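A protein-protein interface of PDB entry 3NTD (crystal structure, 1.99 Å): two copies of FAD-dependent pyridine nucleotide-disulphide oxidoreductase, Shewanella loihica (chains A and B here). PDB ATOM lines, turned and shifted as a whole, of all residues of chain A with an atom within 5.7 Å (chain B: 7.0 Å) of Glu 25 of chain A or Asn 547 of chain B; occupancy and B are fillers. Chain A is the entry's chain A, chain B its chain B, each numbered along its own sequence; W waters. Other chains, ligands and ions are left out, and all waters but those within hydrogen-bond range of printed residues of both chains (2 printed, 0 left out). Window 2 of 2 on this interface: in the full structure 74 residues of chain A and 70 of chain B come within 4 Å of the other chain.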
ATOM      1  N   ALA A  20      -4.887   7.314   8.120  1.00  0.00           N
ATOM      2  CA  ALA A  20      -6.079   6.548   8.079  1.00  0.00           C
ATOM      3  C   ALA A  20      -7.335   7.363   8.410  1.00  0.00           C
ATOM      4  O   ALA A  20      -8.343   7.196   7.741  1.00  0.00           O
ATOM      5  CB  ALA A  20      -5.982   5.311   9.019  1.00  0.00           C
ATOM      6  N   ARG A  21      -7.294   8.266   9.369  1.00  0.00           N
ATOM      7  CA  ARG A  21      -8.465   9.155   9.527  1.00  0.00           C
ATOM      8  C   ARG A  21      -8.708  10.033   8.303  1.00  0.00           C
ATOM      9  O   ARG A  21      -9.830  10.264   7.923  1.00  0.00           O
ATOM     10  CB  ARG A  21      -8.402   9.998  10.841  1.00  0.00           C
ATOM     11  CG  ARG A  21      -9.674  10.854  11.098  1.00  0.00           C
ATOM     12  CD  ARG A  21     -10.968   9.991  11.046  1.00  0.00           C
ATOM     13  NE  ARG A  21     -11.151   9.192  12.279  1.00  0.00           N
ATOM     14  CZ  ARG A  21     -11.655   7.965  12.333  1.00  0.00           C
ATOM     15  NH1 ARG A  21     -12.135   7.381  11.233  1.00  0.00           N
ATOM     16  NH2 ARG A  21     -11.779   7.302  13.500  1.00  0.00           N
ATOM     17  N   LEU A  23      -8.119   9.352   5.352  1.00  0.00           N
ATOM     18  CA  LEU A  23      -8.728   8.474   4.356  1.00  0.00           C
ATOM     19  C   LEU A  23     -10.175   8.097   4.498  1.00  0.00           C
ATOM     20  O   LEU A  23     -10.796   7.767   3.477  1.00  0.00           O
ATOM     21  CB  LEU A  23      -7.922   7.206   4.111  1.00  0.00           C
ATOM     22  CG  LEU A  23      -6.548   7.455   3.471  1.00  0.00           C
ATOM     23  CD1 LEU A  23      -5.695   6.184   3.609  1.00  0.00           C
ATOM     24  CD2 LEU A  23      -6.602   7.884   2.064  1.00  0.00           C
ATOM     25  N   SER A  24     -10.672   7.995   5.747  1.00  0.00           N
ATOM     26  CA  SER A  24     -12.050   7.572   5.982  1.00  0.00           C
ATOM     27  C   SER A  24     -12.470   8.145   7.339  1.00  0.00           C
ATOM     28  O   SER A  24     -11.730   8.001   8.314  1.00  0.00           O
ATOM     29  CB  SER A  24     -12.133   6.031   6.017  1.00  0.00           C
ATOM     30  OG  SER A  24     -13.134   5.531   6.905  1.00  0.00           O
ATOM     31  N   GLU A  25     -13.669   8.750   7.398  1.00  0.00           N
ATOM     32  CA  GLU A  25     -14.323   9.138   8.648  1.00  0.00           C
ATOM     33  C   GLU A  25     -15.130   8.031   9.321  1.00  0.00           C
ATOM     34  O   GLU A  25     -15.431   8.133  10.531  1.00  0.00           O
ATOM     35  CB  GLU A  25     -15.316  10.265   8.363  1.00  0.00           C
ATOM     36  CG  GLU A  25     -14.662  11.633   8.346  1.00  0.00           C
ATOM     37  CD  GLU A  25     -14.013  11.995   9.702  1.00  0.00           C
ATOM     38  OE1 GLU A  25     -14.640  11.816  10.781  1.00  0.00           O
ATOM     39  OE2 GLU A  25     -12.819  12.454   9.681  1.00  0.00           O
ATOM     40  N   THR A  26     -15.521   7.004   8.558  1.00  0.00           N
ATOM     41  CA  THR A  26     -16.253   5.841   9.153  1.00  0.00           C
ATOM     42  C   THR A  26     -15.398   4.747   9.831  1.00  0.00           C
ATOM     43  O   THR A  26     -15.893   4.016  10.706  1.00  0.00           O
ATOM     44  CB  THR A  26     -17.173   5.153   8.132  1.00  0.00           C
ATOM     45  OG1 THR A  26     -16.361   4.640   7.078  1.00  0.00           O
ATOM     46  CG2 THR A  26     -18.268   6.197   7.521  1.00  0.00           C
ATOM     47  N   ALA A  27     -14.114   4.636   9.502  1.00  0.00           N
ATOM     48  CA  ALA A  27     -13.316   3.570  10.199  1.00  0.00           C
ATOM     49  C   ALA A  27     -13.235   3.818  11.730  1.00  0.00           C
ATOM     50  O   ALA A  27     -13.110   4.936  12.156  1.00  0.00           O
ATOM     51  CB  ALA A  27     -11.874   3.492   9.615  1.00  0.00           C
ATOM     52  N   ASN A  72     -10.274  11.911  15.740  1.00  0.00           N
ATOM     53  CA  ASN A  72     -11.195  10.868  16.259  1.00  0.00           C
ATOM     54  C   ASN A  72     -10.564   9.470  16.348  1.00  0.00           C
ATOM     55  O   ASN A  72     -11.180   8.426  15.887  1.00  0.00           O
ATOM     56  CB  ASN A  72     -12.500  10.770  15.484  1.00  0.00           C
ATOM     57  CG  ASN A  72     -13.583   9.920  16.254  1.00  0.00           C
ATOM     58  OD1 ASN A  72     -13.658   9.972  17.516  1.00  0.00           O
ATOM     59  ND2 ASN A  72     -14.453   9.186  15.493  1.00  0.00           N
ATOM     60  N   ARG B 515     -15.242  18.251  13.892  1.00  0.00           N
ATOM     61  CA  ARG B 515     -16.012  17.024  13.728  1.00  0.00           C
ATOM     62  C   ARG B 515     -17.331  17.142  14.495  1.00  0.00           C
ATOM     63  O   ARG B 515     -18.372  16.815  13.946  1.00  0.00           O
ATOM     64  CB  ARG B 515     -15.219  15.775  14.083  1.00  0.00           C
ATOM     65  CG  ARG B 515     -15.958  14.412  14.106  1.00  0.00           C
ATOM     66  CD  ARG B 515     -14.882  13.357  14.468  1.00  0.00           C
ATOM     67  NE  ARG B 515     -13.966  13.260  13.310  1.00  0.00           N
ATOM     68  CZ  ARG B 515     -12.736  13.773  13.263  1.00  0.00           C
ATOM     69  NH1 ARG B 515     -12.216  14.389  14.339  1.00  0.00           N
ATOM     70  NH2 ARG B 515     -12.017  13.654  12.128  1.00  0.00           N
ATOM     71  N   MET B 518     -20.020  20.096  12.929  1.00  0.00           N
ATOM     72  CA  MET B 518     -20.042  20.033  11.494  1.00  0.00           C
ATOM     73  C   MET B 518     -21.412  20.310  10.897  1.00  0.00           C
ATOM     74  O   MET B 518     -21.507  20.776   9.763  1.00  0.00           O
ATOM     75  CB  MET B 518     -19.710  18.640  11.046  1.00  0.00           C
ATOM     76  CG  MET B 518     -19.402  18.580   9.535  1.00  0.00           C
ATOM     77  SD  MET B 518     -18.644  16.962   9.241  1.00  0.00           S
ATOM     78  CE  MET B 518     -18.627  16.738   7.579  1.00  0.00           C
ATOM     79  N   LYS B 523     -24.767  21.529   3.656  1.00  0.00           N
ATOM     80  CA  LYS B 523     -24.194  20.662   2.708  1.00  0.00           C
ATOM     81  C   LYS B 523     -24.511  21.073   1.256  1.00  0.00           C
ATOM     82  O   LYS B 523     -23.881  20.571   0.329  1.00  0.00           O
ATOM     83  CB  LYS B 523     -24.537  19.214   3.071  1.00  0.00           C
ATOM     84  CG  LYS B 523     -24.124  18.185   1.993  1.00  0.00           C
ATOM     85  CD  LYS B 523     -23.433  16.990   2.655  1.00  0.00           C
ATOM     86  CE  LYS B 523     -24.362  16.250   3.525  1.00  0.00           C
ATOM     87  NZ  LYS B 523     -23.732  15.683   4.730  1.00  0.00           N
ATOM     88  N   VAL B 539      -6.612  18.744   6.831  1.00  0.00           N
ATOM     89  CA  VAL B 539      -7.318  17.866   7.834  1.00  0.00           C
ATOM     90  C   VAL B 539      -8.893  18.150   7.771  1.00  0.00           C
ATOM     91  O   VAL B 539      -9.726  17.206   7.670  1.00  0.00           O
ATOM     92  CB  VAL B 539      -6.815  18.120   9.208  1.00  0.00           C
ATOM     93  CG1 VAL B 539      -7.591  17.211  10.239  1.00  0.00           C
ATOM     94  CG2 VAL B 539      -5.279  17.870   9.304  1.00  0.00           C
ATOM     95  N   TYR B 541     -10.581  19.738   5.210  1.00  0.00           N
ATOM     96  CA  TYR B 541     -11.051  19.342   3.906  1.00  0.00           C
ATOM     97  C   TYR B 541     -11.377  17.842   3.893  1.00  0.00           C
ATOM     98  O   TYR B 541     -12.447  17.343   3.342  1.00  0.00           O
ATOM     99  CB  TYR B 541      -9.963  19.651   2.805  1.00  0.00           C
ATOM    100  CG  TYR B 541     -10.218  19.018   1.471  1.00  0.00           C
ATOM    101  CD1 TYR B 541      -9.688  17.772   1.159  1.00  0.00           C
ATOM    102  CD2 TYR B 541     -11.084  19.631   0.534  1.00  0.00           C
ATOM    103  CE1 TYR B 541     -10.020  17.173  -0.046  1.00  0.00           C
ATOM    104  CE2 TYR B 541     -11.384  19.053  -0.674  1.00  0.00           C
ATOM    105  CZ  TYR B 541     -10.839  17.866  -0.984  1.00  0.00           C
ATOM    106  OH  TYR B 541     -11.176  17.247  -2.191  1.00  0.00           O
ATOM    107  N   ARG B 542     -10.452  17.069   4.448  1.00  0.00           N
ATOM    108  CA  ARG B 542     -10.680  15.638   4.424  1.00  0.00           C
ATOM    109  C   ARG B 542     -11.930  15.290   5.210  1.00  0.00           C
ATOM    110  O   ARG B 542     -12.758  14.456   4.728  1.00  0.00           O
ATOM    111  CB  ARG B 542      -9.423  14.878   4.920  1.00  0.00           C
ATOM    112  CG  ARG B 542      -8.256  14.979   3.743  1.00  0.00           C
ATOM    113  CD  ARG B 542      -8.701  14.496   2.354  1.00  0.00           C
ATOM    114  NE  ARG B 542      -9.278  13.121   2.356  1.00  0.00           N
ATOM    115  CZ  ARG B 542      -9.693  12.478   1.271  1.00  0.00           C
ATOM    116  NH1 ARG B 542      -9.499  13.035   0.109  1.00  0.00           N
ATOM    117  NH2 ARG B 542     -10.222  11.250   1.352  1.00  0.00           N
ATOM    118  N   GLN B 543     -12.011  15.775   6.459  1.00  0.00           N
ATOM    119  CA  GLN B 543     -13.223  15.520   7.191  1.00  0.00           C
ATOM    120  C   GLN B 543     -14.543  15.786   6.413  1.00  0.00           C
ATOM    121  O   GLN B 543     -15.426  15.023   6.488  1.00  0.00           O
ATOM    122  CB  GLN B 543     -13.299  16.360   8.436  1.00  0.00           C
ATOM    123  CG  GLN B 543     -12.331  15.901   9.554  1.00  0.00           C
ATOM    124  CD  GLN B 543     -12.678  16.574  10.825  1.00  0.00           C
ATOM    125  OE1 GLN B 543     -13.871  16.767  11.108  1.00  0.00           O
ATOM    126  NE2 GLN B 543     -11.664  16.853  11.666  1.00  0.00           N
ATOM    127  N   LEU B 544     -14.659  16.940   5.777  1.00  0.00           N
ATOM    128  CA  LEU B 544     -15.872  17.318   5.015  1.00  0.00           C
ATOM    129  C   LEU B 544     -16.109  16.545   3.790  1.00  0.00           C
ATOM    130  O   LEU B 544     -17.257  16.209   3.432  1.00  0.00           O
ATOM    131  CB  LEU B 544     -15.829  18.808   4.665  1.00  0.00           C
ATOM    132  CG  LEU B 544     -15.730  19.672   5.900  1.00  0.00           C
ATOM    133  CD1 LEU B 544     -15.263  21.059   5.465  1.00  0.00           C
ATOM    134  CD2 LEU B 544     -16.952  19.746   6.848  1.00  0.00           C
ATOM    135  N   VAL B 545     -15.043  16.201   3.112  1.00  0.00           N
ATOM    136  CA  VAL B 545     -15.178  15.529   1.862  1.00  0.00           C
ATOM    137  C   VAL B 545     -15.497  14.046   2.168  1.00  0.00           C
ATOM    138  O   VAL B 545     -16.285  13.369   1.440  1.00  0.00           O
ATOM    139  CB  VAL B 545     -13.887  15.843   1.100  1.00  0.00           C
ATOM    140  CG1 VAL B 545     -12.922  14.684   0.965  1.00  0.00           C
ATOM    141  CG2 VAL B 545     -14.161  16.725  -0.139  1.00  0.00           C
ATOM    142  N   ASN B 546     -14.946  13.542   3.269  1.00  0.00           N
ATOM    143  CA  ASN B 546     -15.327  12.176   3.624  1.00  0.00           C
ATOM    144  C   ASN B 546     -16.787  12.083   4.100  1.00  0.00           C
ATOM    145  O   ASN B 546     -17.343  10.994   4.214  1.00  0.00           O
ATOM    146  CB  ASN B 546     -14.447  11.649   4.716  1.00  0.00           C
ATOM    147  CG  ASN B 546     -13.094  11.309   4.210  1.00  0.00           C
ATOM    148  OD1 ASN B 546     -12.984  10.850   3.096  1.00  0.00           O
ATOM    149  ND2 ASN B 546     -12.037  11.474   5.055  1.00  0.00           N
ATOM    150  N   ASN B 547     -17.342  13.229   4.466  1.00  0.00           N
ATOM    151  CA  ASN B 547     -18.754  13.320   4.822  1.00  0.00           C
ATOM    152  C   ASN B 547     -19.698  13.763   3.698  1.00  0.00           C
ATOM    153  O   ASN B 547     -20.855  14.103   3.964  1.00  0.00           O
ATOM    154  CB  ASN B 547     -18.890  14.219   6.040  1.00  0.00           C
ATOM    155  CG  ASN B 547     -18.726  13.436   7.304  1.00  0.00           C
ATOM    156  OD1 ASN B 547     -19.590  12.641   7.633  1.00  0.00           O
ATOM    157  ND2 ASN B 547     -17.598  13.597   7.982  1.00  0.00           N
ATOM    158  N   GLY B 548     -19.168  13.776   2.458  1.00  0.00           N
ATOM    159  CA  GLY B 548     -19.933  14.071   1.268  1.00  0.00           C
ATOM    160  C   GLY B 548     -20.177  15.580   1.053  1.00  0.00           C
ATOM    161  O   GLY B 548     -21.067  15.942   0.306  1.00  0.00           O
ATOM    162  N   TYR B 549     -19.394  16.461   1.671  1.00  0.00           N
ATOM    163  CA  TYR B 549     -19.406  17.873   1.247  1.00  0.00           C
ATOM    164  C   TYR B 549     -18.525  18.113  -0.038  1.00  0.00           C
ATOM    165  O   TYR B 549     -17.511  17.401  -0.306  1.00  0.00           O
ATOM    166  CB  TYR B 549     -18.932  18.816   2.355  1.00  0.00           C
ATOM    167  CG  TYR B 549     -19.794  19.005   3.609  1.00  0.00           C
ATOM    168  CD1 TYR B 549     -19.858  18.022   4.600  1.00  0.00           C
ATOM    169  CD2 TYR B 549     -20.486  20.191   3.813  1.00  0.00           C
ATOM    170  CE1 TYR B 549     -20.603  18.218   5.762  1.00  0.00           C
ATOM    171  CE2 TYR B 549     -21.248  20.391   4.957  1.00  0.00           C
ATOM    172  CZ  TYR B 549     -21.306  19.416   5.913  1.00  0.00           C
ATOM    173  OH  TYR B 549     -22.056  19.607   7.048  1.00  0.00           O
HETATM  174  O   HOH W   1     -15.397   8.346   5.277  1.00  0.00           O
HETATM  175  O   HOH W   2     -11.017  12.682   7.640  1.00  0.00           O
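Water W2 lies within hydrogen-bond range of O of Arg 21 of chain A (2.7 Å), OE2 of Glu 25 of chain A (2.7 Å), ND2 of Asn 546 of chain B (3.0 Å) and N of Gln 543 of chain B (3.5 Å). Water W1 lies within hydrogen-bond range of the backbone NH (N) of Glu 25 of chain A and the backbone carbonyl oxygen (O) of Asn 546 of chain B.
Of the 8 printed residues of chain A, 5 touch a printed residue of chain B. Printed residues of chain A that touch a printed residue of chain B: Arg 21, Leu 23, Ser 24, Glu 25 and Asn 72. Of the 13 printed residues of chain B, 4 touch a printed residue of chain A.
The backbone NH (N) of Asn 72 of chain A sits close to the guanidinium group (NH1) of Arg 515 of chain B, at 3.4 Å. The side-chain carboxylate of Glu 25 of chain A lies within salt-bridge range of the guanidinium group of Arg 515 of chain B, 2.8 Å away.
Arg 21 of chain A touches Arg 515 of chain B (CG to NH2, 3.8 Å). Arg 21 of chain A touches Asn 546 of chain B (O to ND2, 3.8 Å). Asn 546 of chain B touches Leu 23 of chain A (OD1 to O, 3.8 Å). Ser 24 of chain A touches Asn 546 of chain B (N to ND2, 3.8 Å). Gln 543 of chain B touches Glu 25 of chain A (CG to OE2, 3.5 Å). Glu 25 of chain A touches Asn 546 of chain B (CG to CB, 3.6 Å). Glu 25 of chain A touches Asn 547 of chain B (CG to ND2, 3.6 Å).
Printed residues of chain B within 4 Å of Glu 25 of chain A: Arg 515, Gln 543, Asn 546 and Asn 547. Asn 547 of chain B touches just one residue of chain A: Glu 25 (3.6 Å). Of the printed residues of chain B, Ser 24 of chain A touches Asn 546. Of the printed residues of chain A, Arg 515 of chain B touches Arg 21, Glu 25 and Asn 72. Of the printed residues of chain A, Gln 543 of chain B touches Glu 25 (3.5 Å). Printed residues of chain B within 4 Å of Leu 23 of chain A: Asn 546 (3.8 Å). Printed residues of chain B within 4 Å of Arg 21 of chain A: Arg 515 and Asn 546. Met 518 of chain B touches none of the printed residues of chain A. Thr 26 of chain A touches none of the printed residues of chain B. The nearest residue of chain B that does not touch Glu 25 of chain A is Arg 542 of chain B (5.0 Å). The nearest printed residue of chain A that does not touch Asn 547 of chain B is Thr 26 of chain A (6.6 Å).
The backbone NH (N) of Ala 27 of chain A is in hydrogen-bond range of the side-chain hydroxyl (OG) of Ser 24 of chain A (2.9 Å). The backbone carbonyl oxygen (O) of Asn 547 of chain B sits at hydrogen-bond distance from the side-chain amino group (NZ) of Lys 523 of chain B (3.4 Å). The backbone carbonyl oxygen (O) of Glu 25 of chain A sits at hydrogen-bond distance from the guanidinium group (NH1) of Arg 21 of chain A, 3.5 Å away. The side-chain amide nitrogen (ND2) of Asn 547 of chain B sits close to the side-chain sulfur (SD) of Met 518 of chain B (3.7 Å). ND2 of Asn 546 of chain B sits at hydrogen-bond distance from O of Arg 542 of chain B. NH1 of Arg 21 of chain A is in hydrogen-bond range of O of Ser 24 of chain A, 3.0 Å away.
No position is printed for both chains.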
